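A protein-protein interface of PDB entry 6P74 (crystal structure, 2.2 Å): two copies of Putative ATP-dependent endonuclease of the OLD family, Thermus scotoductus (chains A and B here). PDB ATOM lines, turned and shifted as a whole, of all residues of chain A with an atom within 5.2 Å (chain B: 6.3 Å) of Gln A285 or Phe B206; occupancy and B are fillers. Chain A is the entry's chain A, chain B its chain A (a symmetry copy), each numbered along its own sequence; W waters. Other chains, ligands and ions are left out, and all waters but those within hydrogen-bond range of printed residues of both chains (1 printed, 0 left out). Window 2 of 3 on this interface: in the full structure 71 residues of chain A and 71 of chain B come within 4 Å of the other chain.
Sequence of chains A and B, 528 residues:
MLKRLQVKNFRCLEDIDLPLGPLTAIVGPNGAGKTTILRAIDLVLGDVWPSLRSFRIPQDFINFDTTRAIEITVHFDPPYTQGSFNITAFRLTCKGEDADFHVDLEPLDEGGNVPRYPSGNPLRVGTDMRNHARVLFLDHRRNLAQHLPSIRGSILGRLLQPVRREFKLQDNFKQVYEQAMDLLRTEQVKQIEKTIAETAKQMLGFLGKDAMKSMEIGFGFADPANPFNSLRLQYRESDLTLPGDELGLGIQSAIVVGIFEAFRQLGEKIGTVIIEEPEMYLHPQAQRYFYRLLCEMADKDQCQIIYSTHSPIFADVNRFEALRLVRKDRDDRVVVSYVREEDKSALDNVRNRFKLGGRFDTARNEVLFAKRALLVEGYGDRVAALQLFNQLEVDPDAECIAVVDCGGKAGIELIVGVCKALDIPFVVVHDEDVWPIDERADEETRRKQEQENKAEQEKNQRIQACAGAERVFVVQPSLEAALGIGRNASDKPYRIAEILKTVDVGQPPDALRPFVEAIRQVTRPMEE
A ring nitrogen (NE2) of His A283 sits close to the backbone carbonyl oxygen (O) of Phe B206, 3.2 Å away.
The backbone NH (N) of Gln A285 lies within hydrogen-bond range of a ring nitrogen (ND1) of His A283 (2.9 Å).
His A283 touches Leu B207 (CD2 to CD2, 3.8 Å).
CB of Gln A285 touches CG of Phe B206, 3.5 Å away.
SD of Met B203 touches CB of Ala A286 (3.7 Å).
N of Ala A286 touches CD2 of Phe B206, 3.5 Å away.
Tyr A289 touches Met B203 (CD1 to SD, 3.5 Å).
Of chain B, only Phe B206 comes within 4 Å of Gln A285.
Of the printed residues of chain B, Ala A286 touches Met B203 and Phe B206.
Of the printed residues of chain A, Leu B207 touches His A283 (3.8 Å).
Of the printed residues of chain A, Met B203 touches Ala A286 and Tyr A289.
Printed residues of chain B within 4 Å of His A283: Phe B206 and Leu B207.
The nearest residue of chain B that does not touch Gln A285 is Met B203 (5.4 Å).
The nearest printed residue of chain A that does not touch Met B203 is His A283 (4.7 Å).
Hydrophobic or aromatic side chains of chain B within 4 Å of the printed part of chain A: Met B203, Phe B206 and Leu B207.
Of the 7 printed residues of chain A, 4 touch a printed residue of chain B.
Hydrophobic or aromatic side chains of chain A that line the printed part of chain B: His A283, Ala A286 and Tyr A289.
No position is printed for both chains.
Water W1 bridges the backbone NH (N) of His A283 and the backbone carbonyl oxygen (O) of Met B203.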
ATOM      1  N   HIS A 283      11.713  21.504  17.828  1.00  0.00           N
ATOM      2  CA  HIS A 283      12.745  22.510  17.675  1.00  0.00           C
ATOM      3  C   HIS A 283      13.584  22.174  16.445  1.00  0.00           C
ATOM      4  O   HIS A 283      13.771  20.996  16.125  1.00  0.00           O
ATOM      5  CB  HIS A 283      13.625  22.553  18.925  1.00  0.00           C
ATOM      6  CG  HIS A 283      14.569  23.713  18.966  1.00  0.00           C
ATOM      7  ND1 HIS A 283      15.746  23.741  18.248  1.00  0.00           N
ATOM      8  CD2 HIS A 283      14.513  24.885  19.642  1.00  0.00           C
ATOM      9  CE1 HIS A 283      16.369  24.888  18.467  1.00  0.00           C
ATOM     10  NE2 HIS A 283      15.647  25.598  19.316  1.00  0.00           N
ATOM     11  N   PRO A 284      14.097  23.188  15.733  1.00  0.00           N
ATOM     12  CA  PRO A 284      15.003  22.906  14.604  1.00  0.00           C
ATOM     13  C   PRO A 284      16.137  21.933  14.937  1.00  0.00           C
ATOM     14  O   PRO A 284      16.503  21.103  14.094  1.00  0.00           O
ATOM     15  CB  PRO A 284      15.543  24.300  14.242  1.00  0.00           C
ATOM     16  CG  PRO A 284      14.452  25.238  14.652  1.00  0.00           C
ATOM     17  CD  PRO A 284      13.783  24.626  15.861  1.00  0.00           C
ATOM     18  N   GLN A 285      16.730  22.049  16.126  1.00  0.00           N
ATOM     19  CA  GLN A 285      17.778  21.121  16.545  1.00  0.00           C
ATOM     20  C   GLN A 285      17.236  19.703  16.665  1.00  0.00           C
ATOM     21  O   GLN A 285      17.926  18.734  16.334  1.00  0.00           O
ATOM     22  CB  GLN A 285      18.371  21.574  17.880  1.00  0.00           C
ATOM     23  CG  GLN A 285      19.806  21.139  18.112  1.00  0.00           C
ATOM     24  CD  GLN A 285      20.785  21.795  17.143  1.00  0.00           C
ATOM     25  OE1 GLN A 285      20.384  22.523  16.235  1.00  0.00           O
ATOM     26  NE2 GLN A 285      22.074  21.537  17.340  1.00  0.00           N
ATOM     27  N   ALA A 286      15.999  19.565  17.142  1.00  0.00           N
ATOM     28  CA  ALA A 286      15.373  18.252  17.208  1.00  0.00           C
ATOM     29  C   ALA A 286      15.005  17.752  15.827  1.00  0.00           C
ATOM     30  O   ALA A 286      15.009  16.538  15.590  1.00  0.00           O
ATOM     31  CB  ALA A 286      14.128  18.287  18.100  1.00  0.00           C
ATOM     32  N   GLN A 287      14.660  18.663  14.919  1.00  0.00           N
ATOM     33  CA  GLN A 287      14.400  18.263  13.548  1.00  0.00           C
ATOM     34  C   GLN A 287      15.659  17.718  12.915  1.00  0.00           C
ATOM     35  O   GLN A 287      15.617  16.735  12.165  1.00  0.00           O
ATOM     36  CB  GLN A 287      13.864  19.444  12.748  1.00  0.00           C
ATOM     37  CG  GLN A 287      12.530  20.002  13.242  1.00  0.00           C
ATOM     38  CD  GLN A 287      12.160  21.251  12.456  1.00  0.00           C
ATOM     39  OE1 GLN A 287      12.429  21.339  11.258  1.00  0.00           O
ATOM     40  NE2 GLN A 287      11.577  22.232  13.132  1.00  0.00           N
ATOM     41  N   ARG A 288      16.797  18.319  13.241  1.00  0.00           N
ATOM     42  CA  ARG A 288      18.055  17.804  12.731  1.00  0.00           C
ATOM     43  C   ARG A 288      18.339  16.429  13.298  1.00  0.00           C
ATOM     44  O   ARG A 288      18.782  15.531  12.576  1.00  0.00           O
ATOM     45  CB  ARG A 288      19.189  18.778  13.046  1.00  0.00           C
ATOM     46  CG  ARG A 288      19.342  19.843  11.981  1.00  0.00           C
ATOM     47  CD  ARG A 288      20.501  20.841  12.250  1.00  0.00           C
ATOM     48  NE  ARG A 288      20.002  22.113  12.777  1.00  0.00           N
ATOM     49  CZ  ARG A 288      19.612  23.146  12.029  1.00  0.00           C
ATOM     50  NH1 ARG A 288      19.681  23.100  10.693  1.00  0.00           N
ATOM     51  NH2 ARG A 288      19.163  24.241  12.629  1.00  0.00           N
ATOM     52  N   TYR A 289      18.076  16.239  14.586  1.00  0.00           N
ATOM     53  CA  TYR A 289      18.289  14.931  15.190  1.00  0.00           C
ATOM     54  C   TYR A 289      17.368  13.879  14.556  1.00  0.00           C
ATOM     55  O   TYR A 289      17.812  12.798  14.169  1.00  0.00           O
ATOM     56  CB  TYR A 289      18.089  15.052  16.708  1.00  0.00           C
ATOM     57  CG  TYR A 289      18.285  13.770  17.459  1.00  0.00           C
ATOM     58  CD1 TYR A 289      17.279  12.835  17.512  1.00  0.00           C
ATOM     59  CD2 TYR A 289      19.475  13.499  18.117  1.00  0.00           C
ATOM     60  CE1 TYR A 289      17.440  11.656  18.183  1.00  0.00           C
ATOM     61  CE2 TYR A 289      19.650  12.312  18.805  1.00  0.00           C
ATOM     62  CZ  TYR A 289      18.617  11.390  18.823  1.00  0.00           C
ATOM     63  OH  TYR A 289      18.737  10.188  19.482  1.00  0.00           O
ATOM     64  N   LYS B 201      13.262  13.818  26.149  1.00  0.00           N
ATOM     65  CA  LYS B 201      13.684  14.916  27.014  1.00  0.00           C
ATOM     66  C   LYS B 201      14.807  15.709  26.374  1.00  0.00           C
ATOM     67  O   LYS B 201      14.866  16.934  26.513  1.00  0.00           O
ATOM     68  CB  LYS B 201      14.107  14.402  28.388  1.00  0.00           C
ATOM     69  CG  LYS B 201      12.948  14.176  29.349  1.00  0.00           C
ATOM     70  CD  LYS B 201      13.479  13.838  30.732  1.00  0.00           C
ATOM     71  CE  LYS B 201      12.360  13.423  31.678  1.00  0.00           C
ATOM     72  NZ  LYS B 201      12.909  13.145  33.040  1.00  0.00           N
ATOM     73  N   GLN B 202      15.705  15.028  25.660  1.00  0.00           N
ATOM     74  CA  GLN B 202      16.749  15.728  24.928  1.00  0.00           C
ATOM     75  C   GLN B 202      16.155  16.588  23.809  1.00  0.00           C
ATOM     76  O   GLN B 202      16.553  17.742  23.624  1.00  0.00           O
ATOM     77  CB  GLN B 202      17.755  14.713  24.382  1.00  0.00           C
ATOM     78  CG  GLN B 202      18.901  15.318  23.595  1.00  0.00           C
ATOM     79  CD  GLN B 202      19.743  14.272  22.891  1.00  0.00           C
ATOM     80  OE1 GLN B 202      19.384  13.092  22.850  1.00  0.00           O
ATOM     81  NE2 GLN B 202      20.869  14.699  22.326  1.00  0.00           N
ATOM     82  N   MET B 203      15.191  16.049  23.058  1.00  0.00           N
ATOM     83  CA  MET B 203      14.519  16.871  22.058  1.00  0.00           C
ATOM     84  C   MET B 203      13.865  18.088  22.701  1.00  0.00           C
ATOM     85  O   MET B 203      13.842  19.168  22.109  1.00  0.00           O
ATOM     86  CB  MET B 203      13.468  16.064  21.292  1.00  0.00           C
ATOM     87  CG  MET B 203      13.973  14.837  20.567  1.00  0.00           C
ATOM     88  SD  MET B 203      15.400  15.077  19.484  1.00  0.00           S
ATOM     89  CE  MET B 203      16.745  14.840  20.621  1.00  0.00           C
ATOM     90  N   LEU B 204      13.294  17.923  23.897  1.00  0.00           N
ATOM     91  CA  LEU B 204      12.623  19.034  24.564  1.00  0.00           C
ATOM     92  C   LEU B 204      13.621  20.015  25.130  1.00  0.00           C
ATOM     93  O   LEU B 204      13.325  21.212  25.224  1.00  0.00           O
ATOM     94  CB  LEU B 204      11.706  18.534  25.682  1.00  0.00           C
ATOM     95  CG  LEU B 204      10.420  17.867  25.177  1.00  0.00           C
ATOM     96  CD1 LEU B 204       9.572  17.378  26.336  1.00  0.00           C
ATOM     97  CD2 LEU B 204       9.624  18.814  24.275  1.00  0.00           C
ATOM     98  N   GLY B 205      14.805  19.527  25.489  1.00  0.00           N
ATOM     99  CA  GLY B 205      15.823  20.395  26.043  1.00  0.00           C
ATOM    100  C   GLY B 205      16.270  21.474  25.079  1.00  0.00           C
ATOM    101  O   GLY B 205      16.668  22.560  25.507  1.00  0.00           O
ATOM    102  N   PHE B 206      16.217  21.191  23.767  1.00  0.00           N
ATOM    103  CA  PHE B 206      16.592  22.190  22.768  1.00  0.00           C
ATOM    104  C   PHE B 206      15.694  23.422  22.820  1.00  0.00           C
ATOM    105  O   PHE B 206      16.091  24.487  22.334  1.00  0.00           O
ATOM    106  CB  PHE B 206      16.539  21.606  21.358  1.00  0.00           C
ATOM    107  CG  PHE B 206      17.501  20.477  21.120  1.00  0.00           C
ATOM    108  CD1 PHE B 206      18.810  20.548  21.566  1.00  0.00           C
ATOM    109  CD2 PHE B 206      17.086  19.331  20.417  1.00  0.00           C
ATOM    110  CE1 PHE B 206      19.703  19.490  21.332  1.00  0.00           C
ATOM    111  CE2 PHE B 206      17.961  18.286  20.169  1.00  0.00           C
ATOM    112  CZ  PHE B 206      19.275  18.358  20.637  1.00  0.00           C
ATOM    113  N   LEU B 207      14.491  23.301  23.385  1.00  0.00           N
ATOM    114  CA  LEU B 207      13.619  24.456  23.556  1.00  0.00           C
ATOM    115  C   LEU B 207      14.121  25.433  24.614  1.00  0.00           C
ATOM    116  O   LEU B 207      13.580  26.543  24.708  1.00  0.00           O
ATOM    117  CB  LEU B 207      12.212  23.980  23.895  1.00  0.00           C
ATOM    118  CG  LEU B 207      11.549  23.207  22.753  1.00  0.00           C
ATOM    119  CD1 LEU B 207      10.236  22.585  23.220  1.00  0.00           C
ATOM    120  CD2 LEU B 207      11.327  24.120  21.535  1.00  0.00           C
ATOM    121  N   GLY B 208      15.143  25.065  25.393  1.00  0.00           N
ATOM    122  CA  GLY B 208      15.724  25.947  26.385  1.00  0.00           C
ATOM    123  C   GLY B 208      14.972  26.025  27.691  1.00  0.00           C
ATOM    124  O   GLY B 208      15.581  26.345  28.719  1.00  0.00           O
ATOM    125  N   LYS B 209      13.668  25.733  27.684  1.00  0.00           N
ATOM    126  CA  LYS B 209      12.821  25.721  28.871  1.00  0.00           C
ATOM    127  C   LYS B 209      13.315  24.709  29.899  1.00  0.00           C
ATOM    128  O   LYS B 209      13.162  23.493  29.711  1.00  0.00           O
ATOM    129  CB  LYS B 209      11.372  25.407  28.477  1.00  0.00           C
ATOM    130  CG  LYS B 209      10.732  26.400  27.503  1.00  0.00           C
ATOM    131  CD  LYS B 209       9.712  25.721  26.581  1.00  0.00           C
ATOM    132  CE  LYS B 209       9.139  24.448  27.206  1.00  0.00           C
ATOM    133  NZ  LYS B 209       8.398  24.700  28.471  1.00  0.00           N
HETATM  134  O   HOH W   1      11.740  19.802  20.100  1.00  0.00           O
